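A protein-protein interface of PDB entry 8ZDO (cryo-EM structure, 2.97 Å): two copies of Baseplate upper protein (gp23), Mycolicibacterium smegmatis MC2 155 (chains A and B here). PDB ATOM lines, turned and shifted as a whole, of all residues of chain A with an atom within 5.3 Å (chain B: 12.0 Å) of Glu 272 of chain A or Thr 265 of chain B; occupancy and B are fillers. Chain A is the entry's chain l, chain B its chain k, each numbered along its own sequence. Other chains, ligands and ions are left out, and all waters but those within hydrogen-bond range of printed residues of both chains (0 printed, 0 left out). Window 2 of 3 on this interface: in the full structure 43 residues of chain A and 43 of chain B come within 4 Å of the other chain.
The backbone carbonyl oxygen (O) of Thr 265 of chain B is in hydrogen-bond range of the side-chain hydroxyl (OH) of Tyr 262 of chain A (2.6 Å). The side-chain hydroxyl (OG1) of Thr 265 of chain B is in hydrogen-bond range of the side-chain carboxylate (OE2) of Glu 272 of chain A, 3.0 Å away. The backbone NH (N) of Leu 267 of chain B sits at hydrogen-bond distance from the backbone carbonyl oxygen (O) of Leu 267 of chain A (2.9 Å).
The backbone carbonyl oxygen of Val 247 of chain B sits at hydrogen-bond distance from the backbone NH of Gly 264 of chain B, 2.8 Å away. O of Lys 263 of chain B lies within hydrogen-bond range of OG of Ser 266 of chain B (3.3 Å). The backbone carbonyl oxygen (O) of Leu 256 of chain A lies within hydrogen-bond range of the side-chain hydroxyl (OG1) of Thr 258 of chain A (2.9 Å). OG1 of Thr 258 of chain A lies within hydrogen-bond range of OG of Ser 274 of chain A (3.3 Å). The side-chain hydroxyl (OH) of Tyr 262 of chain A lies within hydrogen-bond range of the side-chain hydroxyl (OG) of Ser 260 of chain A (3.3 Å).
Among the printed residues, pairs that only touch across the chains: Leu 256 of chain A with Val 247 of chain B (3.7 Å), Leu 256 of chain A with Gly 264 of chain B (3.6 Å), Leu 256 of chain A with Thr 265 of chain B (3.2 Å), Thr 258 of chain A with Thr 265 of chain B (3.9 Å), Ser 260 of chain A with Thr 265 of chain B (3.4 Å), Tyr 262 of chain A with Leu 267 of chain B (3.6 Å), Leu 267 of chain A with Ser 266 of chain B (3.8 Å), Leu 267 of chain A with Thr 268 of chain B (3.9 Å) and Pro 269 of chain A with Thr 265 of chain B (3.5 Å).
Of chain B, only Thr 265 comes within 4 Å of Glu 272 of chain A. Of chain A, only Leu 256 (3.2 Å), Thr 258 (3.9 Å), Ser 260 (3.4 Å), Tyr 262 (2.6 Å), Pro 269 (3.5 Å) and Glu 272 (3.0 Å) come within 4 Å of Thr 265 of chain B. Of chain B, only Thr 265 (3.9 Å) comes within 4 Å of Thr 258 of chain A. No residue of chain B comes within 4 Å of Ile 259 of chain A. Ser 260 of chain A touches just one residue of chain B: Thr 265 (3.4 Å). No residue of chain B comes within 4 Å of Cys 261 of chain A. Pro 269 of chain A touches one residue of chain B. No residue of chain B comes within 4 Å of Ile 271 of chain A. No residue of chain B comes within 4 Å of Ala 273 of chain A. Of the printed residues of chain A, Thr 268 of chain B touches Leu 267. Printed residues of chain B within 4 Å of Leu 267 of chain A: Ser 266, Leu 267 and Thr 268. Printed residues of chain A within 4 Å of Val 247 of chain B: Leu 256 (3.7 Å). Thr 180 of chain B touches none of the printed residues of chain A. Thr 249 of chain B touches none of the printed residues of chain A. The nearest residue of chain A that does not touch Thr 265 of chain B is Leu 267 of chain A (4.9 Å). The nearest printed residue of chain A that does not touch Leu 267 of chain B is Pro 269 of chain A (5.7 Å).
Of the 14 printed residues of chain A, 7 touch a printed residue of chain B. Hydrophobic or aromatic side chains of chain A that line the printed part of chain B: Leu 256, Tyr 262, Leu 267 and Pro 269. Of the 25 printed residues of chain B, 6 touch a printed residue of chain A. Hydrophobic or aromatic side chains of chain B within 4 Å of the printed part of chain A: Val 247 and Leu 267. Along chain B the printed residues that touch a printed residue of chain A span positions 247 to 268.
Tyr 262 of chain A touches Leu 267 of chain B, but with the chains exchanged Leu 267 of chain A does not touch Tyr 262 of chain B (7.2 Å). Leu 267 of chain B touches its own counterpart, Leu 267 of chain A. Positions printed for both chains: 260, 261, 262, 267, 269 and 270. Of the 12 pairs that touch across the chains among the printed residues, 1 has its exchanged pair printed and touching as well.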
ATOM      1  N   VAL A 222      10.960  20.180  -3.753  1.00  0.00           N
ATOM      2  CA  VAL A 222      11.381  18.787  -3.679  1.00  0.00           C
ATOM      3  C   VAL A 222      10.462  18.089  -2.690  1.00  0.00           C
ATOM      4  O   VAL A 222      10.324  18.532  -1.545  1.00  0.00           O
ATOM      5  CB  VAL A 222      12.851  18.652  -3.252  1.00  0.00           C
ATOM      6  CG1 VAL A 222      13.178  17.203  -2.949  1.00  0.00           C
ATOM      7  CG2 VAL A 222      13.768  19.193  -4.328  1.00  0.00           C
ATOM      8  N   LEU A 256      25.504   9.824  -5.102  1.00  0.00           N
ATOM      9  CA  LEU A 256      25.434  11.101  -4.414  1.00  0.00           C
ATOM     10  C   LEU A 256      24.203  11.219  -3.529  1.00  0.00           C
ATOM     11  O   LEU A 256      24.130  12.152  -2.721  1.00  0.00           O
ATOM     12  CB  LEU A 256      25.442  12.243  -5.435  1.00  0.00           C
ATOM     13  CG  LEU A 256      25.923  13.624  -4.993  1.00  0.00           C
ATOM     14  CD1 LEU A 256      27.155  13.514  -4.115  1.00  0.00           C
ATOM     15  CD2 LEU A 256      26.214  14.475  -6.210  1.00  0.00           C
ATOM     16  N   THR A 258      21.326  12.189  -4.302  1.00  0.00           N
ATOM     17  CA  THR A 258      20.916  13.563  -4.559  1.00  0.00           C
ATOM     18  C   THR A 258      19.936  13.619  -5.719  1.00  0.00           C
ATOM     19  O   THR A 258      20.222  13.103  -6.800  1.00  0.00           O
ATOM     20  CB  THR A 258      22.132  14.448  -4.860  1.00  0.00           C
ATOM     21  OG1 THR A 258      22.903  14.625  -3.667  1.00  0.00           O
ATOM     22  CG2 THR A 258      21.693  15.808  -5.372  1.00  0.00           C
ATOM     23  N   ILE A 259      18.799  14.267  -5.501  1.00  0.00           N
ATOM     24  CA  ILE A 259      17.836  14.534  -6.561  1.00  0.00           C
ATOM     25  C   ILE A 259      17.922  16.016  -6.901  1.00  0.00           C
ATOM     26  O   ILE A 259      17.743  16.874  -6.030  1.00  0.00           O
ATOM     27  CB  ILE A 259      16.409  14.131  -6.159  1.00  0.00           C
ATOM     28  CG1 ILE A 259      15.405  14.636  -7.194  1.00  0.00           C
ATOM     29  CG2 ILE A 259      16.070  14.632  -4.763  1.00  0.00           C
ATOM     30  CD1 ILE A 259      14.018  14.081  -7.013  1.00  0.00           C
ATOM     31  N   SER A 260      18.207  16.316  -8.164  1.00  0.00           N
ATOM     32  CA  SER A 260      18.352  17.687  -8.618  1.00  0.00           C
ATOM     33  C   SER A 260      17.498  17.908  -9.854  1.00  0.00           C
ATOM     34  O   SER A 260      17.171  16.969 -10.580  1.00  0.00           O
ATOM     35  CB  SER A 260      19.810  18.025  -8.928  1.00  0.00           C
ATOM     36  OG  SER A 260      20.332  17.157  -9.916  1.00  0.00           O
ATOM     37  N   CYS A 261      17.121  19.162 -10.071  1.00  0.00           N
ATOM     38  CA  CYS A 261      16.358  19.569 -11.240  1.00  0.00           C
ATOM     39  C   CYS A 261      17.069  20.730 -11.913  1.00  0.00           C
ATOM     40  O   CYS A 261      17.382  21.732 -11.259  1.00  0.00           O
ATOM     41  CB  CYS A 261      14.930  19.971 -10.865  1.00  0.00           C
ATOM     42  SG  CYS A 261      13.948  20.570 -12.256  1.00  0.00           S
ATOM     43  N   TYR A 262      17.313  20.581 -13.212  1.00  0.00           N
ATOM     44  CA  TYR A 262      17.888  21.609 -14.067  1.00  0.00           C
ATOM     45  C   TYR A 262      16.824  22.107 -15.031  1.00  0.00           C
ATOM     46  O   TYR A 262      15.985  21.330 -15.498  1.00  0.00           O
ATOM     47  CB  TYR A 262      19.078  21.077 -14.873  1.00  0.00           C
ATOM     48  CG  TYR A 262      20.050  20.211 -14.108  1.00  0.00           C
ATOM     49  CD1 TYR A 262      19.773  18.875 -13.859  1.00  0.00           C
ATOM     50  CD2 TYR A 262      21.255  20.723 -13.659  1.00  0.00           C
ATOM     51  CE1 TYR A 262      20.661  18.083 -13.168  1.00  0.00           C
ATOM     52  CE2 TYR A 262      22.148  19.938 -12.967  1.00  0.00           C
ATOM     53  CZ  TYR A 262      21.847  18.619 -12.725  1.00  0.00           C
ATOM     54  OH  TYR A 262      22.735  17.829 -12.037  1.00  0.00           O
ATOM     55  N   LEU A 267      23.592  24.373 -16.755  1.00  0.00           N
ATOM     56  CA  LEU A 267      24.550  23.441 -16.179  1.00  0.00           C
ATOM     57  C   LEU A 267      24.519  23.424 -14.659  1.00  0.00           C
ATOM     58  O   LEU A 267      25.194  22.588 -14.050  1.00  0.00           O
ATOM     59  CB  LEU A 267      25.966  23.782 -16.654  1.00  0.00           C
ATOM     60  CG  LEU A 267      26.125  24.001 -18.159  1.00  0.00           C
ATOM     61  CD1 LEU A 267      27.578  24.265 -18.512  1.00  0.00           C
ATOM     62  CD2 LEU A 267      25.588  22.808 -18.935  1.00  0.00           C
ATOM     63  N   PRO A 269      22.049  23.125 -11.191  1.00  0.00           N
ATOM     64  CA  PRO A 269      20.705  22.676 -10.807  1.00  0.00           C
ATOM     65  C   PRO A 269      19.817  23.843 -10.406  1.00  0.00           C
ATOM     66  O   PRO A 269      20.203  24.693  -9.602  1.00  0.00           O
ATOM     67  CB  PRO A 269      20.966  21.741  -9.623  1.00  0.00           C
ATOM     68  CG  PRO A 269      22.381  21.340  -9.749  1.00  0.00           C
ATOM     69  CD  PRO A 269      23.105  22.460 -10.413  1.00  0.00           C
ATOM     70  N   LEU A 270      18.614  23.878 -10.981  1.00  0.00           N
ATOM     71  CA  LEU A 270      17.614  24.837 -10.525  1.00  0.00           C
ATOM     72  C   LEU A 270      17.227  24.561  -9.082  1.00  0.00           C
ATOM     73  O   LEU A 270      17.103  25.488  -8.273  1.00  0.00           O
ATOM     74  CB  LEU A 270      16.388  24.789 -11.434  1.00  0.00           C
ATOM     75  CG  LEU A 270      15.130  25.479 -10.914  1.00  0.00           C
ATOM     76  CD1 LEU A 270      15.323  26.984 -10.881  1.00  0.00           C
ATOM     77  CD2 LEU A 270      13.935  25.110 -11.768  1.00  0.00           C
ATOM     78  N   ILE A 271      17.036  23.288  -8.738  1.00  0.00           N
ATOM     79  CA  ILE A 271      16.806  22.878  -7.358  1.00  0.00           C
ATOM     80  C   ILE A 271      17.633  21.631  -7.082  1.00  0.00           C
ATOM     81  O   ILE A 271      18.041  20.917  -7.998  1.00  0.00           O
ATOM     82  CB  ILE A 271      15.311  22.625  -7.053  1.00  0.00           C
ATOM     83  CG1 ILE A 271      15.027  22.834  -5.566  1.00  0.00           C
ATOM     84  CG2 ILE A 271      14.902  21.229  -7.476  1.00  0.00           C
ATOM     85  CD1 ILE A 271      13.563  22.879  -5.225  1.00  0.00           C
ATOM     86  N   GLU A 272      17.884  21.374  -5.801  1.00  0.00           N
ATOM     87  CA  GLU A 272      18.738  20.261  -5.416  1.00  0.00           C
ATOM     88  C   GLU A 272      18.414  19.855  -3.986  1.00  0.00           C
ATOM     89  O   GLU A 272      18.192  20.713  -3.129  1.00  0.00           O
ATOM     90  CB  GLU A 272      20.217  20.642  -5.546  1.00  0.00           C
ATOM     91  CG  GLU A 272      21.196  19.524  -5.255  1.00  0.00           C
ATOM     92  CD  GLU A 272      22.634  19.966  -5.436  1.00  0.00           C
ATOM     93  OE1 GLU A 272      22.850  21.147  -5.778  1.00  0.00           O
ATOM     94  OE2 GLU A 272      23.549  19.138  -5.238  1.00  0.00           O
ATOM     95  N   ALA A 273      18.387  18.547  -3.740  1.00  0.00           N
ATOM     96  CA  ALA A 273      18.177  18.024  -2.398  1.00  0.00           C
ATOM     97  C   ALA A 273      18.962  16.732  -2.250  1.00  0.00           C
ATOM     98  O   ALA A 273      19.223  16.034  -3.233  1.00  0.00           O
ATOM     99  CB  ALA A 273      16.694  17.784  -2.107  1.00  0.00           C
ATOM    100  N   SER A 274      19.335  16.417  -1.012  1.00  0.00           N
ATOM    101  CA  SER A 274      20.172  15.259  -0.738  1.00  0.00           C
ATOM    102  C   SER A 274      19.773  14.634   0.591  1.00  0.00           C
ATOM    103  O   SER A 274      19.193  15.287   1.463  1.00  0.00           O
ATOM    104  CB  SER A 274      21.658  15.637  -0.713  1.00  0.00           C
ATOM    105  OG  SER A 274      22.460  14.527  -0.354  1.00  0.00           O
ATOM    106  N   THR B 180      29.473   5.846 -19.471  1.00  0.00           N
ATOM    107  CA  THR B 180      29.442   6.720 -18.306  1.00  0.00           C
ATOM    108  C   THR B 180      29.875   5.924 -17.084  1.00  0.00           C
ATOM    109  O   THR B 180      29.381   4.818 -16.857  1.00  0.00           O
ATOM    110  CB  THR B 180      28.042   7.300 -18.090  1.00  0.00           C
ATOM    111  OG1 THR B 180      27.602   7.947 -19.289  1.00  0.00           O
ATOM    112  CG2 THR B 180      28.049   8.303 -16.957  1.00  0.00           C
ATOM    113  N   ILE B 181      30.802   6.474 -16.308  1.00  0.00           N
ATOM    114  CA  ILE B 181      31.305   5.830 -15.102  1.00  0.00           C
ATOM    115  C   ILE B 181      31.119   6.794 -13.943  1.00  0.00           C
ATOM    116  O   ILE B 181      31.733   7.865 -13.915  1.00  0.00           O
ATOM    117  CB  ILE B 181      32.782   5.429 -15.242  1.00  0.00           C
ATOM    118  CG1 ILE B 181      33.028   4.738 -16.582  1.00  0.00           C
ATOM    119  CG2 ILE B 181      33.192   4.526 -14.099  1.00  0.00           C
ATOM    120  CD1 ILE B 181      32.532   3.319 -16.636  1.00  0.00           C
ATOM    121  N   VAL B 182      30.285   6.413 -12.984  1.00  0.00           N
ATOM    122  CA  VAL B 182      30.022   7.221 -11.800  1.00  0.00           C
ATOM    123  C   VAL B 182      30.725   6.557 -10.627  1.00  0.00           C
ATOM    124  O   VAL B 182      30.402   5.422 -10.262  1.00  0.00           O
ATOM    125  CB  VAL B 182      28.517   7.368 -11.537  1.00  0.00           C
ATOM    126  CG1 VAL B 182      28.280   8.162 -10.274  1.00  0.00           C
ATOM    127  CG2 VAL B 182      27.841   8.036 -12.719  1.00  0.00           C
ATOM    128  N   VAL B 183      31.691   7.258 -10.041  1.00  0.00           N
ATOM    129  CA  VAL B 183      32.545   6.702  -9.002  1.00  0.00           C
ATOM    130  C   VAL B 183      32.459   7.593  -7.773  1.00  0.00           C
ATOM    131  O   VAL B 183      32.691   8.803  -7.861  1.00  0.00           O
ATOM    132  CB  VAL B 183      34.003   6.576  -9.477  1.00  0.00           C
ATOM    133  CG1 VAL B 183      34.818   5.822  -8.461  1.00  0.00           C
ATOM    134  CG2 VAL B 183      34.069   5.882 -10.821  1.00  0.00           C
ATOM    135  N   ARG B 184      32.132   6.995  -6.633  1.00  0.00           N
ATOM    136  CA  ARG B 184      32.182   7.678  -5.348  1.00  0.00           C
ATOM    137  C   ARG B 184      33.436   7.214  -4.626  1.00  0.00           C
ATOM    138  O   ARG B 184      33.632   6.007  -4.438  1.00  0.00           O
ATOM    139  CB  ARG B 184      30.939   7.388  -4.511  1.00  0.00           C
ATOM    140  CG  ARG B 184      31.006   7.968  -3.108  1.00  0.00           C
ATOM    141  CD  ARG B 184      29.889   7.441  -2.232  1.00  0.00           C
ATOM    142  NE  ARG B 184      29.905   8.054  -0.911  1.00  0.00           N
ATOM    143  CZ  ARG B 184      30.645   7.628   0.104  1.00  0.00           C
ATOM    144  NH1 ARG B 184      31.445   6.582  -0.016  1.00  0.00           N
ATOM    145  NH2 ARG B 184      30.578   8.268   1.268  1.00  0.00           N
ATOM    146  N   ASN B 240      41.815  20.296  -8.209  1.00  0.00           N
ATOM    147  CA  ASN B 240      40.629  19.635  -7.673  1.00  0.00           C
ATOM    148  C   ASN B 240      40.980  19.027  -6.328  1.00  0.00           C
ATOM    149  O   ASN B 240      41.862  18.166  -6.251  1.00  0.00           O
ATOM    150  CB  ASN B 240      40.123  18.559  -8.631  1.00  0.00           C
ATOM    151  CG  ASN B 240      38.859  17.886  -8.135  1.00  0.00           C
ATOM    152  OD1 ASN B 240      38.201  18.370  -7.216  1.00  0.00           O
ATOM    153  ND2 ASN B 240      38.520  16.753  -8.737  1.00  0.00           N
ATOM    154  N   THR B 241      40.298  19.466  -5.277  1.00  0.00           N
ATOM    155  CA  THR B 241      40.402  18.840  -3.970  1.00  0.00           C
ATOM    156  C   THR B 241      39.269  17.833  -3.822  1.00  0.00           C
ATOM    157  O   THR B 241      38.125  18.115  -4.195  1.00  0.00           O
ATOM    158  CB  THR B 241      40.373  19.883  -2.847  1.00  0.00           C
ATOM    159  OG1 THR B 241      40.644  19.250  -1.590  1.00  0.00           O
ATOM    160  CG2 THR B 241      39.034  20.611  -2.783  1.00  0.00           C
ATOM    161  N   GLY B 245      33.448  10.806   0.123  1.00  0.00           N
ATOM    162  CA  GLY B 245      32.115  10.796  -0.439  1.00  0.00           C
ATOM    163  C   GLY B 245      31.943  11.594  -1.709  1.00  0.00           C
ATOM    164  O   GLY B 245      30.803  11.810  -2.135  1.00  0.00           O
ATOM    165  N   ASP B 246      33.031  12.048  -2.323  1.00  0.00           N
ATOM    166  CA  ASP B 246      32.928  12.795  -3.566  1.00  0.00           C
ATOM    167  C   ASP B 246      32.554  11.871  -4.716  1.00  0.00           C
ATOM    168  O   ASP B 246      33.092  10.769  -4.853  1.00  0.00           O
ATOM    169  CB  ASP B 246      34.242  13.509  -3.872  1.00  0.00           C
ATOM    170  CG  ASP B 246      34.270  14.926  -3.344  1.00  0.00           C
ATOM    171  OD1 ASP B 246      33.403  15.269  -2.514  1.00  0.00           O
ATOM    172  OD2 ASP B 246      35.159  15.699  -3.757  1.00  0.00           O
ATOM    173  N   VAL B 247      31.634  12.336  -5.557  1.00  0.00           N
ATOM    174  CA  VAL B 247      31.116  11.569  -6.682  1.00  0.00           C
ATOM    175  C   VAL B 247      31.568  12.240  -7.970  1.00  0.00           C
ATOM    176  O   VAL B 247      31.353  13.442  -8.161  1.00  0.00           O
ATOM    177  CB  VAL B 247      29.582  11.458  -6.624  1.00  0.00           C
ATOM    178  CG1 VAL B 247      29.055  10.751  -7.855  1.00  0.00           C
ATOM    179  CG2 VAL B 247      29.157  10.725  -5.366  1.00  0.00           C
ATOM    180  N   TYR B 248      32.197  11.464  -8.849  1.00  0.00           N
ATOM    181  CA  TYR B 248      32.706  11.949 -10.123  1.00  0.00           C
ATOM    182  C   TYR B 248      32.099  11.142 -11.260  1.00  0.00           C
ATOM    183  O   TYR B 248      31.968   9.918 -11.167  1.00  0.00           O
ATOM    184  CB  TYR B 248      34.231  11.853 -10.181  1.00  0.00           C
ATOM    185  CG  TYR B 248      34.936  12.739  -9.186  1.00  0.00           C
ATOM    186  CD1 TYR B 248      35.216  14.061  -9.486  1.00  0.00           C
ATOM    187  CD2 TYR B 248      35.324  12.250  -7.947  1.00  0.00           C
ATOM    188  CE1 TYR B 248      35.862  14.873  -8.581  1.00  0.00           C
ATOM    189  CE2 TYR B 248      35.968  13.055  -7.036  1.00  0.00           C
ATOM    190  CZ  TYR B 248      36.234  14.367  -7.357  1.00  0.00           C
ATOM    191  OH  TYR B 248      36.878  15.175  -6.451  1.00  0.00           O
ATOM    192  N   THR B 249      31.737  11.832 -12.336  1.00  0.00           N
ATOM    193  CA  THR B 249      31.119  11.219 -13.506  1.00  0.00           C
ATOM    194  C   THR B 249      32.066  11.380 -14.689  1.00  0.00           C
ATOM    195  O   THR B 249      32.275  12.495 -15.174  1.00  0.00           O
ATOM    196  CB  THR B 249      29.763  11.853 -13.799  1.00  0.00           C
ATOM    197  OG1 THR B 249      29.010  11.958 -12.585  1.00  0.00           O
ATOM    198  CG2 THR B 249      28.989  11.016 -14.792  1.00  0.00           C
ATOM    199  N   ILE B 250      32.631  10.272 -15.150  1.00  0.00           N
ATOM    200  CA  ILE B 250      33.521  10.247 -16.304  1.00  0.00           C
ATOM    201  C   ILE B 250      32.707   9.755 -17.491  1.00  0.00           C
ATOM    202  O   ILE B 250      32.302   8.591 -17.538  1.00  0.00           O
ATOM    203  CB  ILE B 250      34.743   9.353 -16.058  1.00  0.00           C
ATOM    204  CG1 ILE B 250      35.623   9.934 -14.951  1.00  0.00           C
ATOM    205  CG2 ILE B 250      35.539   9.177 -17.338  1.00  0.00           C
ATOM    206  CD1 ILE B 250      35.323   9.389 -13.577  1.00  0.00           C
ATOM    207  N   LYS B 251      32.467  10.633 -18.454  1.00  0.00           N
ATOM    208  CA  LYS B 251      31.679  10.308 -19.634  1.00  0.00           C
ATOM    209  C   LYS B 251      32.578  10.329 -20.859  1.00  0.00           C
ATOM    210  O   LYS B 251      33.244  11.334 -21.130  1.00  0.00           O
ATOM    211  CB  LYS B 251      30.520  11.289 -19.806  1.00  0.00           C
ATOM    212  CG  LYS B 251      29.440  11.161 -18.756  1.00  0.00           C
ATOM    213  CD  LYS B 251      28.332  12.173 -18.977  1.00  0.00           C
ATOM    214  CE  LYS B 251      27.261  12.046 -17.909  1.00  0.00           C
ATOM    215  NZ  LYS B 251      26.185  13.059 -18.068  1.00  0.00           N
ATOM    216  N   SER B 260      35.277  13.396 -20.776  1.00  0.00           N
ATOM    217  CA  SER B 260      34.996  14.489 -19.861  1.00  0.00           C
ATOM    218  C   SER B 260      34.777  13.943 -18.461  1.00  0.00           C
ATOM    219  O   SER B 260      34.361  12.797 -18.283  1.00  0.00           O
ATOM    220  CB  SER B 260      33.769  15.288 -20.308  1.00  0.00           C
ATOM    221  OG  SER B 260      33.431  16.272 -19.348  1.00  0.00           O
ATOM    222  N   CYS B 261      35.069  14.776 -17.469  1.00  0.00           N
ATOM    223  CA  CYS B 261      34.828  14.444 -16.076  1.00  0.00           C
ATOM    224  C   CYS B 261      34.084  15.593 -15.421  1.00  0.00           C
ATOM    225  O   CYS B 261      34.493  16.755 -15.540  1.00  0.00           O
ATOM    226  CB  CYS B 261      36.132  14.156 -15.329  1.00  0.00           C
ATOM    227  SG  CYS B 261      35.912  13.705 -13.595  1.00  0.00           S
ATOM    228  N   TYR B 262      32.992  15.255 -14.739  1.00  0.00           N
ATOM    229  CA  TYR B 262      32.154  16.187 -14.003  1.00  0.00           C
ATOM    230  C   TYR B 262      32.193  15.825 -12.526  1.00  0.00           C
ATOM    231  O   TYR B 262      32.341  14.655 -12.165  1.00  0.00           O
ATOM    232  CB  TYR B 262      30.701  16.150 -14.496  1.00  0.00           C
ATOM    233  CG  TYR B 262      30.540  16.131 -16.000  1.00  0.00           C
ATOM    234  CD1 TYR B 262      30.664  14.949 -16.717  1.00  0.00           C
ATOM    235  CD2 TYR B 262      30.245  17.289 -16.700  1.00  0.00           C
ATOM    236  CE1 TYR B 262      30.515  14.928 -18.089  1.00  0.00           C
ATOM    237  CE2 TYR B 262      30.094  17.277 -18.072  1.00  0.00           C
ATOM    238  CZ  TYR B 262      30.228  16.095 -18.758  1.00  0.00           C
ATOM    239  OH  TYR B 262      30.074  16.081 -20.125  1.00  0.00           O
ATOM    240  N   LYS B 263      32.052  16.831 -11.672  1.00  0.00           N
ATOM    241  CA  LYS B 263      32.141  16.646 -10.232  1.00  0.00           C
ATOM    242  C   LYS B 263      30.797  16.939  -9.584  1.00  0.00           C
ATOM    243  O   LYS B 263      30.171  17.962  -9.877  1.00  0.00           O
ATOM    244  CB  LYS B 263      33.218  17.547  -9.630  1.00  0.00           C
ATOM    245  CG  LYS B 263      33.409  17.360  -8.136  1.00  0.00           C
ATOM    246  CD  LYS B 263      34.562  18.196  -7.624  1.00  0.00           C
ATOM    247  CE  LYS B 263      34.948  17.788  -6.215  1.00  0.00           C
ATOM    248  NZ  LYS B 263      33.782  17.817  -5.292  1.00  0.00           N
ATOM    249  N   GLY B 264      30.365  16.042  -8.703  1.00  0.00           N
ATOM    250  CA  GLY B 264      29.160  16.287  -7.930  1.00  0.00           C
ATOM    251  C   GLY B 264      27.925  16.355  -8.802  1.00  0.00           C
ATOM    252  O   GLY B 264      27.635  15.444  -9.585  1.00  0.00           O
ATOM    253  N   THR B 265      27.184  17.451  -8.667  1.00  0.00           N
ATOM    254  CA  THR B 265      25.906  17.611  -9.344  1.00  0.00           C
ATOM    255  C   THR B 265      25.980  18.558 -10.537  1.00  0.00           C
ATOM    256  O   THR B 265      25.127  18.478 -11.428  1.00  0.00           O
ATOM    257  CB  THR B 265      24.855  18.113  -8.343  1.00  0.00           C
ATOM    258  OG1 THR B 265      24.820  17.230  -7.216  1.00  0.00           O
ATOM    259  CG2 THR B 265      23.475  18.116  -8.955  1.00  0.00           C
ATOM    260  N   SER B 266      26.990  19.422 -10.595  1.00  0.00           N
ATOM    261  CA  SER B 266      27.109  20.367 -11.698  1.00  0.00           C
ATOM    262  C   SER B 266      27.366  19.638 -13.011  1.00  0.00           C
ATOM    263  O   SER B 266      28.102  18.650 -13.060  1.00  0.00           O
ATOM    264  CB  SER B 266      28.235  21.363 -11.427  1.00  0.00           C
ATOM    265  OG  SER B 266      29.500  20.744 -11.567  1.00  0.00           O
ATOM    266  N   LEU B 267      26.751  20.133 -14.081  1.00  0.00           N
ATOM    267  CA  LEU B 267      26.885  19.537 -15.402  1.00  0.00           C
ATOM    268  C   LEU B 267      28.001  20.158 -16.228  1.00  0.00           C
ATOM    269  O   LEU B 267      28.225  19.725 -17.362  1.00  0.00           O
ATOM    270  CB  LEU B 267      25.563  19.646 -16.167  1.00  0.00           C
ATOM    271  CG  LEU B 267      24.421  18.769 -15.658  1.00  0.00           C
ATOM    272  CD1 LEU B 267      23.125  19.122 -16.361  1.00  0.00           C
ATOM    273  CD2 LEU B 267      24.752  17.299 -15.845  1.00  0.00           C
ATOM    274  N   THR B 268      28.695  21.160 -15.703  1.00  0.00           N
ATOM    275  CA  THR B 268      29.830  21.716 -16.421  1.00  0.00           C
ATOM    276  C   THR B 268      31.019  20.761 -16.332  1.00  0.00           C
ATOM    277  O   THR B 268      31.285  20.194 -15.268  1.00  0.00           O
ATOM    278  CB  THR B 268      30.206  23.093 -15.869  1.00  0.00           C
ATOM    279  OG1 THR B 268      31.386  23.568 -16.525  1.00  0.00           O
ATOM    280  CG2 THR B 268      30.443  23.038 -14.368  1.00  0.00           C
ATOM    281  N   PRO B 269      31.735  20.541 -17.435  1.00  0.00           N
ATOM    282  CA  PRO B 269      32.855  19.588 -17.419  1.00  0.00           C
ATOM    283  C   PRO B 269      33.982  20.084 -16.527  1.00  0.00           C
ATOM    284  O   PRO B 269      34.592  21.120 -16.796  1.00  0.00           O
ATOM    285  CB  PRO B 269      33.286  19.521 -18.890  1.00  0.00           C
ATOM    286  CG  PRO B 269      32.097  19.992 -19.657  1.00  0.00           C
ATOM    287  CD  PRO B 269      31.451  21.030 -18.793  1.00  0.00           C
ATOM    288  N   LEU B 270      34.250  19.337 -15.453  1.00  0.00           N
ATOM    289  CA  LEU B 270      35.390  19.662 -14.600  1.00  0.00           C
ATOM    290  C   LEU B 270      36.695  19.539 -15.374  1.00  0.00           C
ATOM    291  O   LEU B 270      37.585  20.388 -15.242  1.00  0.00           O
ATOM    292  CB  LEU B 270      35.402  18.760 -13.368  1.00  0.00           C
ATOM    293  CG  LEU B 270      36.707  18.670 -12.580  1.00  0.00           C
ATOM    294  CD1 LEU B 270      36.973  19.973 -11.848  1.00  0.00           C
ATOM    295  CD2 LEU B 270      36.656  17.507 -11.607  1.00  0.00           C
